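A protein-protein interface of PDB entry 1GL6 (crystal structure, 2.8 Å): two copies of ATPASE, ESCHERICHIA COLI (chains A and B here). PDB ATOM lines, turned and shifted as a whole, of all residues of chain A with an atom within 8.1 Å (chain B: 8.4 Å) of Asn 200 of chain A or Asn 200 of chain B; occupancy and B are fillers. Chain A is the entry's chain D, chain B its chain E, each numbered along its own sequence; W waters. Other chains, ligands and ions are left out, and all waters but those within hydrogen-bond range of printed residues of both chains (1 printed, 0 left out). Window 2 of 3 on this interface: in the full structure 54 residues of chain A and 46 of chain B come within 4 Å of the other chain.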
ATOM      1  N   PHE A 180       5.068  31.526 -26.203  1.00  0.00           N
ATOM      2  CA  PHE A 180       3.834  31.725 -25.483  1.00  0.00           C
ATOM      3  C   PHE A 180       3.594  33.184 -25.169  1.00  0.00           C
ATOM      4  O   PHE A 180       2.506  33.695 -25.403  1.00  0.00           O
ATOM      5  CB  PHE A 180       3.863  30.942 -24.188  1.00  0.00           C
ATOM      6  CG  PHE A 180       2.712  30.015 -24.027  1.00  0.00           C
ATOM      7  CD1 PHE A 180       2.505  28.992 -24.939  1.00  0.00           C
ATOM      8  CD2 PHE A 180       1.849  30.147 -22.949  1.00  0.00           C
ATOM      9  CE1 PHE A 180       1.455  28.113 -24.775  1.00  0.00           C
ATOM     10  CE2 PHE A 180       0.795  29.270 -22.778  1.00  0.00           C
ATOM     11  CZ  PHE A 180       0.597  28.251 -23.691  1.00  0.00           C
ATOM     12  N   ARG A 184       0.757  35.791 -26.493  1.00  0.00           N
ATOM     13  CA  ARG A 184      -0.062  36.429 -25.465  1.00  0.00           C
ATOM     14  C   ARG A 184      -0.072  37.929 -25.675  1.00  0.00           C
ATOM     15  O   ARG A 184      -1.104  38.585 -25.530  1.00  0.00           O
ATOM     16  CB  ARG A 184       0.503  36.136 -24.075  1.00  0.00           C
ATOM     17  CG  ARG A 184       0.139  34.790 -23.477  1.00  0.00           C
ATOM     18  CD  ARG A 184      -0.958  34.950 -22.439  1.00  0.00           C
ATOM     19  NE  ARG A 184      -1.246  33.695 -21.753  1.00  0.00           N
ATOM     20  CZ  ARG A 184      -0.333  32.943 -21.147  1.00  0.00           C
ATOM     21  NH1 ARG A 184      -0.689  31.812 -20.547  1.00  0.00           N
ATOM     22  NH2 ARG A 184       0.938  33.322 -21.140  1.00  0.00           N
ATOM     23  N   PHE A 196      -7.025  33.147 -22.437  1.00  0.00           N
ATOM     24  CA  PHE A 196      -5.921  32.205 -22.403  1.00  0.00           C
ATOM     25  C   PHE A 196      -4.907  32.568 -21.353  1.00  0.00           C
ATOM     26  O   PHE A 196      -3.742  32.226 -21.474  1.00  0.00           O
ATOM     27  CB  PHE A 196      -5.239  32.139 -23.760  1.00  0.00           C
ATOM     28  CG  PHE A 196      -5.983  31.321 -24.770  1.00  0.00           C
ATOM     29  CD1 PHE A 196      -6.358  31.877 -25.982  1.00  0.00           C
ATOM     30  CD2 PHE A 196      -6.293  29.986 -24.523  1.00  0.00           C
ATOM     31  CE1 PHE A 196      -7.026  31.121 -26.928  1.00  0.00           C
ATOM     32  CE2 PHE A 196      -6.964  29.226 -25.471  1.00  0.00           C
ATOM     33  CZ  PHE A 196      -7.328  29.794 -26.673  1.00  0.00           C
ATOM     34  N   ALA A 197      -5.337  33.266 -20.320  1.00  0.00           N
ATOM     35  CA  ALA A 197      -4.412  33.630 -19.275  1.00  0.00           C
ATOM     36  C   ALA A 197      -5.113  33.591 -17.920  1.00  0.00           C
ATOM     37  O   ALA A 197      -6.348  33.579 -17.846  1.00  0.00           O
ATOM     38  CB  ALA A 197      -3.848  35.011 -19.550  1.00  0.00           C
ATOM     39  N   GLY A 198      -4.328  33.540 -16.848  1.00  0.00           N
ATOM     40  CA  GLY A 198      -4.922  33.552 -15.523  1.00  0.00           C
ATOM     41  C   GLY A 198      -4.837  32.302 -14.672  1.00  0.00           C
ATOM     42  O   GLY A 198      -5.034  32.373 -13.459  1.00  0.00           O
ATOM     43  N   SER A 199      -4.563  31.154 -15.278  1.00  0.00           N
ATOM     44  CA  SER A 199      -4.460  29.922 -14.501  1.00  0.00           C
ATOM     45  C   SER A 199      -3.756  28.858 -15.307  1.00  0.00           C
ATOM     46  O   SER A 199      -3.423  29.072 -16.468  1.00  0.00           O
ATOM     47  CB  SER A 199      -5.841  29.412 -14.124  1.00  0.00           C
ATOM     48  OG  SER A 199      -6.538  29.023 -15.290  1.00  0.00           O
ATOM     49  N   ASN A 200      -3.513  27.708 -14.698  1.00  0.00           N
ATOM     50  CA  ASN A 200      -2.863  26.637 -15.434  1.00  0.00           C
ATOM     51  C   ASN A 200      -3.827  26.181 -16.513  1.00  0.00           C
ATOM     52  O   ASN A 200      -3.420  25.852 -17.626  1.00  0.00           O
ATOM     53  CB  ASN A 200      -2.533  25.465 -14.516  1.00  0.00           C
ATOM     54  CG  ASN A 200      -1.477  25.814 -13.484  1.00  0.00           C
ATOM     55  OD1 ASN A 200      -0.345  26.151 -13.834  1.00  0.00           O
ATOM     56  ND2 ASN A 200      -1.842  25.739 -12.206  1.00  0.00           N
ATOM     57  N   GLU A 201      -5.110  26.169 -16.173  1.00  0.00           N
ATOM     58  CA  GLU A 201      -6.127  25.759 -17.120  1.00  0.00           C
ATOM     59  C   GLU A 201      -6.067  26.652 -18.371  1.00  0.00           C
ATOM     60  O   GLU A 201      -6.042  26.156 -19.497  1.00  0.00           O
ATOM     61  CB  GLU A 201      -7.502  25.823 -16.455  1.00  0.00           C
ATOM     62  CG  GLU A 201      -8.626  25.230 -17.279  1.00  0.00           C
ATOM     63  CD  GLU A 201      -8.399  23.770 -17.618  1.00  0.00           C
ATOM     64  OE1 GLU A 201      -9.218  23.212 -18.377  1.00  0.00           O
ATOM     65  OE2 GLU A 201      -7.410  23.175 -17.132  1.00  0.00           O
ATOM     66  N   ALA A 202      -6.016  27.966 -18.180  1.00  0.00           N
ATOM     67  CA  ALA A 202      -5.931  28.910 -19.294  1.00  0.00           C
ATOM     68  C   ALA A 202      -4.724  28.625 -20.211  1.00  0.00           C
ATOM     69  O   ALA A 202      -4.824  28.687 -21.437  1.00  0.00           O
ATOM     70  CB  ALA A 202      -5.841  30.331 -18.744  1.00  0.00           C
ATOM     71  N   SER A 203      -3.583  28.325 -19.595  1.00  0.00           N
ATOM     72  CA  SER A 203      -2.347  28.044 -20.316  1.00  0.00           C
ATOM     73  C   SER A 203      -2.440  26.692 -20.983  1.00  0.00           C
ATOM     74  O   SER A 203      -1.848  26.463 -22.032  1.00  0.00           O
ATOM     75  CB  SER A 203      -1.153  28.035 -19.357  1.00  0.00           C
ATOM     76  OG  SER A 203      -0.788  29.339 -18.946  1.00  0.00           O
ATOM     77  N   LYS A 204      -3.167  25.785 -20.351  1.00  0.00           N
ATOM     78  CA  LYS A 204      -3.332  24.460 -20.902  1.00  0.00           C
ATOM     79  C   LYS A 204      -4.127  24.621 -22.182  1.00  0.00           C
ATOM     80  O   LYS A 204      -3.757  24.091 -23.232  1.00  0.00           O
ATOM     81  CB  LYS A 204      -4.102  23.598 -19.924  1.00  0.00           C
ATOM     82  CG  LYS A 204      -4.288  22.175 -20.365  1.00  0.00           C
ATOM     83  CD  LYS A 204      -5.306  21.499 -19.481  1.00  0.00           C
ATOM     84  CE  LYS A 204      -5.625  20.111 -19.979  1.00  0.00           C
ATOM     85  NZ  LYS A 204      -6.773  19.548 -19.217  1.00  0.00           N
ATOM     86  N   ALA A 205      -5.221  25.370 -22.076  1.00  0.00           N
ATOM     87  CA  ALA A 205      -6.108  25.648 -23.198  1.00  0.00           C
ATOM     88  C   ALA A 205      -5.334  26.197 -24.382  1.00  0.00           C
ATOM     89  O   ALA A 205      -5.530  25.763 -25.513  1.00  0.00           O
ATOM     90  CB  ALA A 205      -7.175  26.642 -22.777  1.00  0.00           C
ATOM     91  N   LEU A 206      -4.450  27.151 -24.115  1.00  0.00           N
ATOM     92  CA  LEU A 206      -3.654  27.756 -25.170  1.00  0.00           C
ATOM     93  C   LEU A 206      -2.797  26.699 -25.846  1.00  0.00           C
ATOM     94  O   LEU A 206      -2.758  26.621 -27.068  1.00  0.00           O
ATOM     95  CB  LEU A 206      -2.765  28.852 -24.590  1.00  0.00           C
ATOM     96  CG  LEU A 206      -2.682  30.124 -25.423  1.00  0.00           C
ATOM     97  CD1 LEU A 206      -1.510  30.953 -24.941  1.00  0.00           C
ATOM     98  CD2 LEU A 206      -2.560  29.767 -26.894  1.00  0.00           C
ATOM     99  N   THR A 207      -2.120  25.880 -25.043  1.00  0.00           N
ATOM    100  CA  THR A 207      -1.259  24.811 -25.542  1.00  0.00           C
ATOM    101  C   THR A 207      -2.015  23.836 -26.439  1.00  0.00           C
ATOM    102  O   THR A 207      -1.460  23.313 -27.410  1.00  0.00           O
ATOM    103  CB  THR A 207      -0.655  24.014 -24.370  1.00  0.00           C
ATOM    104  OG1 THR A 207       0.343  24.810 -23.730  1.00  0.00           O
ATOM    105  CG2 THR A 207      -0.027  22.705 -24.858  1.00  0.00           C
ATOM    106  N   PHE B 180      15.735  17.170 -20.823  1.00  0.00           N
ATOM    107  CA  PHE B 180      14.646  17.955 -21.361  1.00  0.00           C
ATOM    108  C   PHE B 180      15.104  19.254 -22.017  1.00  0.00           C
ATOM    109  O   PHE B 180      14.672  19.581 -23.129  1.00  0.00           O
ATOM    110  CB  PHE B 180      13.646  18.250 -20.251  1.00  0.00           C
ATOM    111  CG  PHE B 180      12.220  17.933 -20.623  1.00  0.00           C
ATOM    112  CD1 PHE B 180      11.879  16.677 -21.140  1.00  0.00           C
ATOM    113  CD2 PHE B 180      11.212  18.878 -20.424  1.00  0.00           C
ATOM    114  CE1 PHE B 180      10.558  16.366 -21.451  1.00  0.00           C
ATOM    115  CE2 PHE B 180       9.892  18.578 -20.732  1.00  0.00           C
ATOM    116  CZ  PHE B 180       9.562  17.317 -21.246  1.00  0.00           C
ATOM    117  N   ARG B 184      15.023  20.396 -25.817  1.00  0.00           N
ATOM    118  CA  ARG B 184      14.332  21.668 -26.041  1.00  0.00           C
ATOM    119  C   ARG B 184      15.191  22.581 -26.914  1.00  0.00           C
ATOM    120  O   ARG B 184      14.705  23.200 -27.863  1.00  0.00           O
ATOM    121  CB  ARG B 184      14.077  22.356 -24.706  1.00  0.00           C
ATOM    122  CG  ARG B 184      12.888  21.829 -23.951  1.00  0.00           C
ATOM    123  CD  ARG B 184      11.674  22.705 -24.199  1.00  0.00           C
ATOM    124  NE  ARG B 184      10.502  22.268 -23.438  1.00  0.00           N
ATOM    125  CZ  ARG B 184      10.476  22.081 -22.120  1.00  0.00           C
ATOM    126  NH1 ARG B 184       9.352  21.688 -21.537  1.00  0.00           N
ATOM    127  NH2 ARG B 184      11.567  22.278 -21.388  1.00  0.00           N
ATOM    128  N   PHE B 196       6.255  22.284 -27.680  1.00  0.00           N
ATOM    129  CA  PHE B 196       6.557  21.558 -26.445  1.00  0.00           C
ATOM    130  C   PHE B 196       7.062  22.429 -25.308  1.00  0.00           C
ATOM    131  O   PHE B 196       7.820  21.963 -24.465  1.00  0.00           O
ATOM    132  CB  PHE B 196       7.592  20.461 -26.696  1.00  0.00           C
ATOM    133  CG  PHE B 196       7.060  19.294 -27.454  1.00  0.00           C
ATOM    134  CD1 PHE B 196       7.670  18.882 -28.636  1.00  0.00           C
ATOM    135  CD2 PHE B 196       5.917  18.629 -27.015  1.00  0.00           C
ATOM    136  CE1 PHE B 196       7.147  17.831 -29.376  1.00  0.00           C
ATOM    137  CE2 PHE B 196       5.387  17.578 -27.748  1.00  0.00           C
ATOM    138  CZ  PHE B 196       5.999  17.175 -28.933  1.00  0.00           C
ATOM    139  N   ALA B 197       6.646  23.688 -25.277  1.00  0.00           N
ATOM    140  CA  ALA B 197       7.065  24.593 -24.218  1.00  0.00           C
ATOM    141  C   ALA B 197       5.970  25.620 -23.943  1.00  0.00           C
ATOM    142  O   ALA B 197       5.081  25.837 -24.772  1.00  0.00           O
ATOM    143  CB  ALA B 197       8.361  25.298 -24.617  1.00  0.00           C
ATOM    144  N   GLY B 198       6.031  26.248 -22.774  1.00  0.00           N
ATOM    145  CA  GLY B 198       5.044  27.258 -22.447  1.00  0.00           C
ATOM    146  C   GLY B 198       4.049  26.947 -21.341  1.00  0.00           C
ATOM    147  O   GLY B 198       3.362  27.846 -20.862  1.00  0.00           O
ATOM    148  N   SER B 199       3.952  25.688 -20.929  1.00  0.00           N
ATOM    149  CA  SER B 199       3.016  25.325 -19.865  1.00  0.00           C
ATOM    150  C   SER B 199       3.292  23.914 -19.410  1.00  0.00           C
ATOM    151  O   SER B 199       4.090  23.204 -20.014  1.00  0.00           O
ATOM    152  CB  SER B 199       1.564  25.421 -20.349  1.00  0.00           C
ATOM    153  OG  SER B 199       1.273  24.414 -21.307  1.00  0.00           O
ATOM    154  N   ASN B 200       2.633  23.504 -18.337  1.00  0.00           N
ATOM    155  CA  ASN B 200       2.830  22.150 -17.851  1.00  0.00           C
ATOM    156  C   ASN B 200       2.320  21.210 -18.928  1.00  0.00           C
ATOM    157  O   ASN B 200       2.915  20.167 -19.177  1.00  0.00           O
ATOM    158  CB  ASN B 200       2.057  21.922 -16.557  1.00  0.00           C
ATOM    159  CG  ASN B 200       2.466  22.875 -15.469  1.00  0.00           C
ATOM    160  OD1 ASN B 200       3.649  22.966 -15.123  1.00  0.00           O
ATOM    161  ND2 ASN B 200       1.490  23.595 -14.913  1.00  0.00           N
ATOM    162  N   GLU B 201       1.219  21.592 -19.572  1.00  0.00           N
ATOM    163  CA  GLU B 201       0.618  20.786 -20.630  1.00  0.00           C
ATOM    164  C   GLU B 201       1.674  20.470 -21.696  1.00  0.00           C
ATOM    165  O   GLU B 201       1.933  19.300 -22.004  1.00  0.00           O
ATOM    166  CB  GLU B 201      -0.572  21.544 -21.242  1.00  0.00           C
ATOM    167  CG  GLU B 201      -1.331  20.789 -22.315  1.00  0.00           C
ATOM    168  CD  GLU B 201      -1.924  19.470 -21.834  1.00  0.00           C
ATOM    169  OE1 GLU B 201      -2.340  18.679 -22.699  1.00  0.00           O
ATOM    170  OE2 GLU B 201      -1.987  19.212 -20.614  1.00  0.00           O
ATOM    171  N   ALA B 202       2.302  21.515 -22.227  1.00  0.00           N
ATOM    172  CA  ALA B 202       3.331  21.357 -23.241  1.00  0.00           C
ATOM    173  C   ALA B 202       4.446  20.419 -22.785  1.00  0.00           C
ATOM    174  O   ALA B 202       4.944  19.606 -23.562  1.00  0.00           O
ATOM    175  CB  ALA B 202       3.911  22.719 -23.604  1.00  0.00           C
ATOM    176  N   SER B 203       4.847  20.527 -21.526  1.00  0.00           N
ATOM    177  CA  SER B 203       5.913  19.666 -21.019  1.00  0.00           C
ATOM    178  C   SER B 203       5.403  18.247 -20.911  1.00  0.00           C
ATOM    179  O   SER B 203       6.146  17.295 -21.137  1.00  0.00           O
ATOM    180  CB  SER B 203       6.392  20.152 -19.644  1.00  0.00           C
ATOM    181  OG  SER B 203       7.155  21.341 -19.750  1.00  0.00           O
ATOM    182  N   LYS B 204       4.129  18.117 -20.567  1.00  0.00           N
ATOM    183  CA  LYS B 204       3.511  16.820 -20.405  1.00  0.00           C
ATOM    184  C   LYS B 204       3.534  16.151 -21.754  1.00  0.00           C
ATOM    185  O   LYS B 204       3.911  14.982 -21.877  1.00  0.00           O
ATOM    186  CB  LYS B 204       2.078  16.972 -19.934  1.00  0.00           C
ATOM    187  CG  LYS B 204       1.371  15.671 -19.709  1.00  0.00           C
ATOM    188  CD  LYS B 204      -0.120  15.880 -19.522  1.00  0.00           C
ATOM    189  CE  LYS B 204      -0.867  14.550 -19.438  1.00  0.00           C
ATOM    190  NZ  LYS B 204      -2.336  14.742 -19.272  1.00  0.00           N
ATOM    191  N   ALA B 205       3.140  16.908 -22.772  1.00  0.00           N
ATOM    192  CA  ALA B 205       3.122  16.391 -24.135  1.00  0.00           C
ATOM    193  C   ALA B 205       4.503  15.894 -24.533  1.00  0.00           C
ATOM    194  O   ALA B 205       4.635  14.845 -25.143  1.00  0.00           O
ATOM    195  CB  ALA B 205       2.668  17.464 -25.101  1.00  0.00           C
ATOM    196  N   LEU B 206       5.535  16.646 -24.179  1.00  0.00           N
ATOM    197  CA  LEU B 206       6.891  16.247 -24.511  1.00  0.00           C
ATOM    198  C   LEU B 206       7.222  14.932 -23.806  1.00  0.00           C
ATOM    199  O   LEU B 206       7.728  13.999 -24.420  1.00  0.00           O
ATOM    200  CB  LEU B 206       7.882  17.339 -24.094  1.00  0.00           C
ATOM    201  CG  LEU B 206       9.017  17.608 -25.088  1.00  0.00           C
ATOM    202  CD1 LEU B 206      10.161  18.293 -24.366  1.00  0.00           C
ATOM    203  CD2 LEU B 206       9.508  16.293 -25.717  1.00  0.00           C
ATOM    204  N   THR B 207       6.921  14.862 -22.515  1.00  0.00           N
ATOM    205  CA  THR B 207       7.173  13.669 -21.718  1.00  0.00           C
ATOM    206  C   THR B 207       6.496  12.428 -22.288  1.00  0.00           C
ATOM    207  O   THR B 207       7.053  11.333 -22.252  1.00  0.00           O
ATOM    208  CB  THR B 207       6.680  13.875 -20.284  1.00  0.00           C
ATOM    209  OG1 THR B 207       7.476  14.890 -19.659  1.00  0.00           O
ATOM    210  CG2 THR B 207       6.766  12.572 -19.485  1.00  0.00           C
ATOM    211  N   SER B 208       5.288  12.608 -22.811  1.00  0.00           N
ATOM    212  CA  SER B 208       4.508  11.510 -23.383  1.00  0.00           C
ATOM    213  C   SER B 208       5.182  11.067 -24.669  1.00  0.00           C
ATOM    214  O   SER B 208       5.300   9.868 -24.960  1.00  0.00           O
ATOM    215  CB  SER B 208       3.084  11.987 -23.682  1.00  0.00           C
ATOM    216  OG  SER B 208       2.459  12.542 -22.531  1.00  0.00           O
HETATM  217  O   HOH W   1      -0.737  24.223 -17.870  1.00  0.00           O
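Asn 200 of chain A touches just one residue of chain B: Asn 200 (3.3 Å). Of chain A, only Asn 200 (3.3 Å) comes within 4 Å of Asn 200 of chain B. Of the printed residues of chain B, Ser 203 of chain A touches Ser 199. Of the printed residues of chain B, Thr 207 of chain A touches Ser 199, Glu 201 and Ala 202. Of the printed residues of chain A, Gly 198 of chain B touches Phe 180. Of the printed residues of chain B, Lys 204 of chain A touches Glu 201 (3.8 Å). Ala 205 of chain A touches none of the printed residues of chain B. Arg 184 of chain B touches none of the printed residues of chain A. The nearest printed residue of chain B that does not touch Ser 203 of chain A is Gly 198 of chain B (4.8 Å).
NH1 of Arg 184 of chain A sits at hydrogen-bond distance from OG of Ser 203 of chain A (2.9 Å). The side-chain hydroxyl (OG1) of Thr 207 of chain A lies within hydrogen-bond range of the backbone carbonyl oxygen (O) of Ser 203 of chain A (3.2 Å). The backbone NH of Glu 201 of chain B lies close to the side-chain hydroxyl of Ser 199 of chain B (3.3 Å). The side-chain hydroxyl (OG) of Ser 199 of chain B lies within hydrogen-bond range of the backbone NH (N) of Ala 202 of chain B (3.2 Å).
The side-chain amide oxygen of Asn 200 of chain A lies within hydrogen-bond range of the side-chain amide nitrogen of Asn 200 of chain B (3.3 Å). OG1 of Thr 207 of chain A sits at hydrogen-bond distance from OG of Ser 199 of chain B.
CD2 of Phe 180 of chain A touches O of Gly 198 of chain B, 3.5 Å away. Ser 203 of chain A touches Ser 199 of chain B (O to OG, 3.8 Å). Glu 201 of chain B touches Lys 204 of chain A. CG2 of Thr 207 of chain A touches CG of Glu 201 of chain B, at 3.4 Å. N of Ala 202 of chain B touches CG2 of Thr 207 of chain A, at 3.7 Å.
Water W1 lies within hydrogen-bond range of the backbone carbonyl oxygen of Asn 200 of chain A and the backbone NH of Asn 200 of chain B.
Ser 203 of chain A touches Ser 199 of chain B, but with the chains exchanged Ser 199 of chain A does not touch Ser 203 of chain B (12.9 Å). Lys 204 of chain A touches Glu 201 of chain B, but with the chains exchanged Glu 201 of chain A does not touch Lys 204 of chain B (10.1 Å). Thr 207 of chain A touches Ser 199 of chain B, but with the chains exchanged Ser 199 of chain A does not touch Thr 207 of chain B (18.2 Å). Thr 207 of chain A touches Ala 202 of chain B, but with the chains exchanged Ala 202 of chain A does not touch Thr 207 of chain B (18.2 Å). Of the 7 pairs that touch across the chains among the printed residues, 1 has its exchanged pair printed and touching as well.
Of the 15 printed residues of chain B, 5 touch a printed residue of chain A. Printed residues of chain B that touch a printed residue of chain A: Gly 198, Ser 199, Asn 200, Glu 201 and Ala 202. Printed residues of chain A that touch a printed residue of chain B: Phe 180, Asn 200, Ser 203, Lys 204 and Thr 207. Hydrophobic or aromatic side chains of chain A that line the printed part of chain B: Phe 180. Among the printed residues, no Asp or Glu carboxylate lies within 4 Å of a Lys or Arg side-chain nitrogen of the other chain.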
